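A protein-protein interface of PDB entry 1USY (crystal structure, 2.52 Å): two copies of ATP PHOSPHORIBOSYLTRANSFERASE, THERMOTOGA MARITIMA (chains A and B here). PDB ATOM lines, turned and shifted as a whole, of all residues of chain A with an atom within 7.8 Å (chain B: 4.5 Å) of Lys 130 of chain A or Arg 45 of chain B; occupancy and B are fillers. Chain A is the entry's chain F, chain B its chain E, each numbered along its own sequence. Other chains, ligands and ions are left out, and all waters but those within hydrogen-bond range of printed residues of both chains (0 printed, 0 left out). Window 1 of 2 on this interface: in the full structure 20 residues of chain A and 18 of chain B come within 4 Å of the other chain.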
ATOM      1  N   ARG A  45      12.468  -4.175 -11.873  1.00  0.00           N
ATOM      2  CA  ARG A  45      12.827  -4.519 -13.245  1.00  0.00           C
ATOM      3  C   ARG A  45      13.262  -5.986 -13.299  1.00  0.00           C
ATOM      4  O   ARG A  45      13.832  -6.504 -12.322  1.00  0.00           O
ATOM      5  CB  ARG A  45      13.930  -3.608 -13.759  1.00  0.00           C
ATOM      6  CG  ARG A  45      13.421  -2.258 -14.181  1.00  0.00           C
ATOM      7  CD  ARG A  45      12.707  -2.282 -15.521  1.00  0.00           C
ATOM      8  NE  ARG A  45      13.179  -1.227 -16.423  1.00  0.00           N
ATOM      9  CZ  ARG A  45      13.829  -1.437 -17.581  1.00  0.00           C
ATOM     10  NH1 ARG A  45      14.146  -2.686 -17.986  1.00  0.00           N
ATOM     11  NH2 ARG A  45      14.153  -0.377 -18.334  1.00  0.00           N
ATOM     12  N   THR A 107      24.711  -7.223 -27.185  1.00  0.00           N
ATOM     13  CA  THR A 107      23.616  -7.789 -26.366  1.00  0.00           C
ATOM     14  C   THR A 107      23.146  -6.810 -25.348  1.00  0.00           C
ATOM     15  O   THR A 107      23.953  -6.068 -24.801  1.00  0.00           O
ATOM     16  CB  THR A 107      24.054  -8.995 -25.570  1.00  0.00           C
ATOM     17  OG1 THR A 107      25.456  -8.979 -25.399  1.00  0.00           O
ATOM     18  CG2 THR A 107      23.681 -10.302 -26.219  1.00  0.00           C
ATOM     19  N   LYS A 108      21.984  -7.181 -24.782  1.00  0.00           N
ATOM     20  CA  LYS A 108      21.595  -6.825 -23.410  1.00  0.00           C
ATOM     21  C   LYS A 108      22.104  -7.860 -22.400  1.00  0.00           C
ATOM     22  O   LYS A 108      21.922  -7.695 -21.198  1.00  0.00           O
ATOM     23  CB  LYS A 108      20.077  -6.791 -23.258  1.00  0.00           C
ATOM     24  CG  LYS A 108      19.305  -5.793 -24.047  1.00  0.00           C
ATOM     25  CD  LYS A 108      17.857  -5.814 -23.572  1.00  0.00           C
ATOM     26  CE  LYS A 108      17.282  -7.233 -23.597  1.00  0.00           C
ATOM     27  NZ  LYS A 108      16.288  -7.525 -24.710  1.00  0.00           N
ATOM     28  N   PHE A 109      22.685  -8.951 -22.870  1.00  0.00           N
ATOM     29  CA  PHE A 109      23.166 -10.042 -21.975  1.00  0.00           C
ATOM     30  C   PHE A 109      24.672 -10.304 -22.073  1.00  0.00           C
ATOM     31  O   PHE A 109      25.050 -11.391 -22.489  1.00  0.00           O
ATOM     32  CB  PHE A 109      22.414 -11.367 -22.265  1.00  0.00           C
ATOM     33  CG  PHE A 109      20.909 -11.201 -22.357  1.00  0.00           C
ATOM     34  CD1 PHE A 109      20.329 -10.776 -23.528  1.00  0.00           C
ATOM     35  CD2 PHE A 109      20.094 -11.458 -21.264  1.00  0.00           C
ATOM     36  CE1 PHE A 109      18.970 -10.573 -23.619  1.00  0.00           C
ATOM     37  CE2 PHE A 109      18.726 -11.257 -21.343  1.00  0.00           C
ATOM     38  CZ  PHE A 109      18.161 -10.818 -22.531  1.00  0.00           C
ATOM     39  N   PRO A 110      25.520  -9.348 -21.667  1.00  0.00           N
ATOM     40  CA  PRO A 110      26.983  -9.515 -21.761  1.00  0.00           C
ATOM     41  C   PRO A 110      27.431 -10.842 -21.127  1.00  0.00           C
ATOM     42  O   PRO A 110      28.268 -11.549 -21.692  1.00  0.00           O
ATOM     43  CB  PRO A 110      27.538  -8.335 -20.940  1.00  0.00           C
ATOM     44  CG  PRO A 110      26.351  -7.834 -20.125  1.00  0.00           C
ATOM     45  CD  PRO A 110      25.155  -8.077 -21.003  1.00  0.00           C
ATOM     46  N   ILE A 127      29.807  -5.505 -26.903  1.00  0.00           N
ATOM     47  CA  ILE A 127      29.275  -4.146 -26.854  1.00  0.00           C
ATOM     48  C   ILE A 127      27.969  -4.258 -26.107  1.00  0.00           C
ATOM     49  O   ILE A 127      26.995  -4.787 -26.652  1.00  0.00           O
ATOM     50  CB  ILE A 127      29.027  -3.603 -28.295  1.00  0.00           C
ATOM     51  CG1 ILE A 127      30.197  -3.915 -29.238  1.00  0.00           C
ATOM     52  CG2 ILE A 127      28.710  -2.117 -28.285  1.00  0.00           C
ATOM     53  CD1 ILE A 127      31.426  -3.080 -29.011  1.00  0.00           C
ATOM     54  N   PRO A 128      27.924  -3.817 -24.854  1.00  0.00           N
ATOM     55  CA  PRO A 128      26.691  -3.930 -24.058  1.00  0.00           C
ATOM     56  C   PRO A 128      25.618  -2.908 -24.483  1.00  0.00           C
ATOM     57  O   PRO A 128      25.939  -1.750 -24.676  1.00  0.00           O
ATOM     58  CB  PRO A 128      27.162  -3.665 -22.627  1.00  0.00           C
ATOM     59  CG  PRO A 128      28.626  -3.359 -22.694  1.00  0.00           C
ATOM     60  CD  PRO A 128      29.020  -3.182 -24.110  1.00  0.00           C
ATOM     61  N   LEU A 129      24.375  -3.325 -24.668  1.00  0.00           N
ATOM     62  CA  LEU A 129      23.349  -2.356 -25.029  1.00  0.00           C
ATOM     63  C   LEU A 129      22.175  -2.556 -24.129  1.00  0.00           C
ATOM     64  O   LEU A 129      22.132  -3.532 -23.346  1.00  0.00           O
ATOM     65  CB  LEU A 129      22.933  -2.473 -26.505  1.00  0.00           C
ATOM     66  CG  LEU A 129      24.034  -2.224 -27.522  1.00  0.00           C
ATOM     67  CD1 LEU A 129      23.622  -2.586 -28.936  1.00  0.00           C
ATOM     68  CD2 LEU A 129      24.458  -0.766 -27.446  1.00  0.00           C
ATOM     69  N   LYS A 130      21.239  -1.615 -24.207  1.00  0.00           N
ATOM     70  CA  LYS A 130      20.032  -1.647 -23.370  1.00  0.00           C
ATOM     71  C   LYS A 130      18.729  -2.041 -24.116  1.00  0.00           C
ATOM     72  O   LYS A 130      17.732  -2.352 -23.479  1.00  0.00           O
ATOM     73  CB  LYS A 130      19.885  -0.317 -22.621  1.00  0.00           C
ATOM     74  CG  LYS A 130      20.622  -0.286 -21.266  1.00  0.00           C
ATOM     75  CD  LYS A 130      22.159  -0.364 -21.461  1.00  0.00           C
ATOM     76  CE  LYS A 130      22.896  -0.850 -20.210  1.00  0.00           C
ATOM     77  NZ  LYS A 130      24.362  -0.776 -20.406  1.00  0.00           N
ATOM     78  N   GLY A 131      18.769  -2.044 -25.453  1.00  0.00           N
ATOM     79  CA  GLY A 131      17.614  -2.248 -26.314  1.00  0.00           C
ATOM     80  C   GLY A 131      18.063  -1.974 -27.748  1.00  0.00           C
ATOM     81  O   GLY A 131      19.233  -1.725 -27.987  1.00  0.00           O
ATOM     82  N   SER A 132      17.140  -2.029 -28.705  1.00  0.00           N
ATOM     83  CA  SER A 132      17.452  -1.778 -30.119  1.00  0.00           C
ATOM     84  C   SER A 132      18.719  -2.459 -30.555  1.00  0.00           C
ATOM     85  O   SER A 132      19.429  -1.934 -31.417  1.00  0.00           O
ATOM     86  CB  SER A 132      17.606  -0.301 -30.371  1.00  0.00           C
ATOM     87  OG  SER A 132      16.432   0.386 -30.027  1.00  0.00           O
ATOM     88  N   VAL A 133      18.998  -3.628 -29.965  1.00  0.00           N
ATOM     89  CA  VAL A 133      20.248  -4.329 -30.217  1.00  0.00           C
ATOM     90  C   VAL A 133      20.383  -4.805 -31.662  1.00  0.00           C
ATOM     91  O   VAL A 133      21.475  -5.030 -32.140  1.00  0.00           O
ATOM     92  CB  VAL A 133      20.544  -5.439 -29.127  1.00  0.00           C
ATOM     93  CG1 VAL A 133      19.307  -5.830 -28.358  1.00  0.00           C
ATOM     94  CG2 VAL A 133      21.195  -6.647 -29.692  1.00  0.00           C
ATOM     95  N   LEU A 135      20.031  -3.207 -34.226  1.00  0.00           N
ATOM     96  CA  LEU A 135      20.591  -2.160 -35.050  1.00  0.00           C
ATOM     97  C   LEU A 135      22.075  -2.315 -35.214  1.00  0.00           C
ATOM     98  O   LEU A 135      22.621  -1.854 -36.217  1.00  0.00           O
ATOM     99  CB  LEU A 135      20.356  -0.795 -34.409  1.00  0.00           C
ATOM    100  CG  LEU A 135      18.967  -0.194 -34.431  1.00  0.00           C
ATOM    101  CD1 LEU A 135      19.040   1.080 -33.651  1.00  0.00           C
ATOM    102  CD2 LEU A 135      18.433   0.054 -35.897  1.00  0.00           C
ATOM    103  N   ASP A 147      20.476 -11.944 -28.927  1.00  0.00           N
ATOM    104  CA  ASP A 147      19.250 -11.358 -28.412  1.00  0.00           C
ATOM    105  C   ASP A 147      18.111 -12.335 -28.444  1.00  0.00           C
ATOM    106  O   ASP A 147      18.197 -13.402 -29.040  1.00  0.00           O
ATOM    107  CB  ASP A 147      18.843 -10.108 -29.215  1.00  0.00           C
ATOM    108  CG  ASP A 147      18.080  -9.059 -28.355  1.00  0.00           C
ATOM    109  OD1 ASP A 147      18.368  -8.908 -27.131  1.00  0.00           O
ATOM    110  OD2 ASP A 147      17.185  -8.314 -28.834  1.00  0.00           O
ATOM    111  N   LYS B   8      14.864   6.653 -27.457  1.00  0.00           N
ATOM    112  CA  LYS B   8      13.518   6.174 -27.183  1.00  0.00           C
ATOM    113  C   LYS B   8      13.088   6.598 -25.789  1.00  0.00           C
ATOM    114  O   LYS B   8      13.889   6.579 -24.860  1.00  0.00           O
ATOM    115  CB  LYS B   8      13.453   4.652 -27.298  1.00  0.00           C
ATOM    116  CG  LYS B   8      13.342   4.165 -28.710  1.00  0.00           C
ATOM    117  CD  LYS B   8      12.707   2.788 -28.733  1.00  0.00           C
ATOM    118  CE  LYS B   8      12.800   2.176 -30.103  1.00  0.00           C
ATOM    119  NZ  LYS B   8      11.811   2.831 -31.020  1.00  0.00           N
ATOM    120  N   VAL B  44      17.302   4.446 -30.473  1.00  0.00           N
ATOM    121  CA  VAL B  44      18.051   3.697 -29.478  1.00  0.00           C
ATOM    122  C   VAL B  44      17.689   4.091 -28.027  1.00  0.00           C
ATOM    123  O   VAL B  44      17.117   5.127 -27.780  1.00  0.00           O
ATOM    124  CB  VAL B  44      19.604   3.749 -29.750  1.00  0.00           C
ATOM    125  CG1 VAL B  44      19.957   4.114 -31.194  1.00  0.00           C
ATOM    126  CG2 VAL B  44      20.300   4.711 -28.868  1.00  0.00           C
ATOM    127  N   ARG B  45      18.054   3.259 -27.075  1.00  0.00           N
ATOM    128  CA  ARG B  45      17.866   3.558 -25.666  1.00  0.00           C
ATOM    129  C   ARG B  45      18.840   4.673 -25.257  1.00  0.00           C
ATOM    130  O   ARG B  45      19.987   4.653 -25.713  1.00  0.00           O
ATOM    131  CB  ARG B  45      18.078   2.269 -24.869  1.00  0.00           C
ATOM    132  CG  ARG B  45      17.295   2.170 -23.541  1.00  0.00           C
ATOM    133  CD  ARG B  45      15.860   1.675 -23.616  1.00  0.00           C
ATOM    134  NE  ARG B  45      15.311   1.848 -24.955  1.00  0.00           N
ATOM    135  CZ  ARG B  45      14.861   0.858 -25.723  1.00  0.00           C
ATOM    136  NH1 ARG B  45      14.868  -0.397 -25.278  1.00  0.00           N
ATOM    137  NH2 ARG B  45      14.394   1.117 -26.943  1.00  0.00           N
ATOM    138  N   PRO B  46      18.385   5.664 -24.458  1.00  0.00           N
ATOM    139  CA  PRO B  46      19.205   6.845 -24.071  1.00  0.00           C
ATOM    140  C   PRO B  46      20.648   6.649 -23.613  1.00  0.00           C
ATOM    141  O   PRO B  46      21.479   7.471 -24.031  1.00  0.00           O
ATOM    142  CB  PRO B  46      18.392   7.513 -22.982  1.00  0.00           C
ATOM    143  CG  PRO B  46      16.945   7.194 -23.363  1.00  0.00           C
ATOM    144  CD  PRO B  46      16.993   5.784 -23.965  1.00  0.00           C
ATOM    145  N   PHE B  47      20.954   5.613 -22.819  1.00  0.00           N
ATOM    146  CA  PHE B  47      22.332   5.323 -22.381  1.00  0.00           C
ATOM    147  C   PHE B  47      23.283   5.027 -23.528  1.00  0.00           C
ATOM    148  O   PHE B  47      24.486   5.146 -23.377  1.00  0.00           O
ATOM    149  CB  PHE B  47      22.363   4.084 -21.497  1.00  0.00           C
ATOM    150  CG  PHE B  47      22.371   4.360 -20.030  1.00  0.00           C
ATOM    151  CD1 PHE B  47      21.235   4.882 -19.386  1.00  0.00           C
ATOM    152  CD2 PHE B  47      23.476   4.008 -19.266  1.00  0.00           C
ATOM    153  CE1 PHE B  47      21.222   5.112 -17.990  1.00  0.00           C
ATOM    154  CE2 PHE B  47      23.482   4.227 -17.888  1.00  0.00           C
ATOM    155  CZ  PHE B  47      22.344   4.783 -17.244  1.00  0.00           C
ATOM    156  N   ASP B  48      22.759   4.584 -24.655  1.00  0.00           N
ATOM    157  CA  ASP B  48      23.619   4.080 -25.738  1.00  0.00           C
ATOM    158  C   ASP B  48      23.891   5.125 -26.801  1.00  0.00           C
ATOM    159  O   ASP B  48      24.528   4.804 -27.783  1.00  0.00           O
ATOM    160  CB  ASP B  48      22.968   2.859 -26.429  1.00  0.00           C
ATOM    161  CG  ASP B  48      22.732   1.671 -25.473  1.00  0.00           C
ATOM    162  OD1 ASP B  48      23.595   1.415 -24.589  1.00  0.00           O
ATOM    163  OD2 ASP B  48      21.721   0.935 -25.535  1.00  0.00           O
ATOM    164  N   VAL B  49      23.353   6.342 -26.640  1.00  0.00           N
ATOM    165  CA  VAL B  49      23.537   7.413 -27.618  1.00  0.00           C
ATOM    166  C   VAL B  49      25.034   7.762 -27.708  1.00  0.00           C
ATOM    167  O   VAL B  49      25.581   7.848 -28.804  1.00  0.00           O
ATOM    168  CB  VAL B  49      22.702   8.701 -27.294  1.00  0.00           C
ATOM    169  CG1 VAL B  49      23.210   9.879 -28.091  1.00  0.00           C
ATOM    170  CG2 VAL B  49      21.209   8.519 -27.592  1.00  0.00           C
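OD2 of Asp 48 of chain B lies within hydrogen-bond range of N of Lys 130 of chain A (2.9 Å).
The backbone NH (N) of Lys 8 of chain B lies within hydrogen-bond range of the backbone carbonyl oxygen (O) of Val 44 of chain B, at 2.7 Å. The backbone carbonyl oxygen of Thr 107 of chain A lies within hydrogen-bond range of the backbone NH of Leu 129 of chain A, at 2.8 Å.
Among the printed residues, pairs that only touch across the chains: Gly 131 of chain A with Arg 45 of chain B, Leu 129 of chain A with Asp 48 of chain B, Lys 130 of chain A with Arg 45 of chain B, Ser 132 of chain A with Val 44 of chain B, Ser 132 of chain A with Arg 45 of chain B and Pro 128 of chain A with Asp 48 of chain B.
Arg 45 of chain A touches none of the printed residues of chain B. Thr 107 of chain A touches none of the printed residues of chain B. Printed residues of chain B within 4 Å of Pro 128 of chain A: Asp 48 (3.9 Å). Lys 130 of chain A touches just these residues of chain B: Arg 45 (3.7 Å) and Asp 48 (2.9 Å). Printed residues of chain B within 4 Å of Gly 131 of chain A: Arg 45. Printed residues of chain B within 4 Å of Ser 132 of chain A: Val 44 (3.7 Å) and Arg 45 (3.8 Å). Of the printed residues of chain A, Val 44 of chain B touches Ser 132 (3.7 Å). Arg 45 of chain B touches three residues of chain A. No residue of chain A comes within 4 Å of Pro 46 of chain B. Of the printed residues of chain A, Asp 48 of chain B touches Pro 128, Leu 129 and Lys 130. The nearest printed residue of chain B that does not touch Lys 130 of chain A is Phe 47 of chain B (4.5 Å). The nearest printed residue of chain B that does not touch Leu 129 of chain A is Arg 45 of chain B (6.4 Å).
Of the 14 printed residues of chain A, 5 touch a printed residue of chain B. Of the 7 printed residues of chain B, 3 touch a printed residue of chain A. Printed residues of chain B that touch a printed residue of chain A: Val 44, Arg 45 and Asp 48.
1 position is printed for both chains. Of the 7 pairs that touch across the chains among the printed residues, none has its exchanged pair printed and touching as well.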
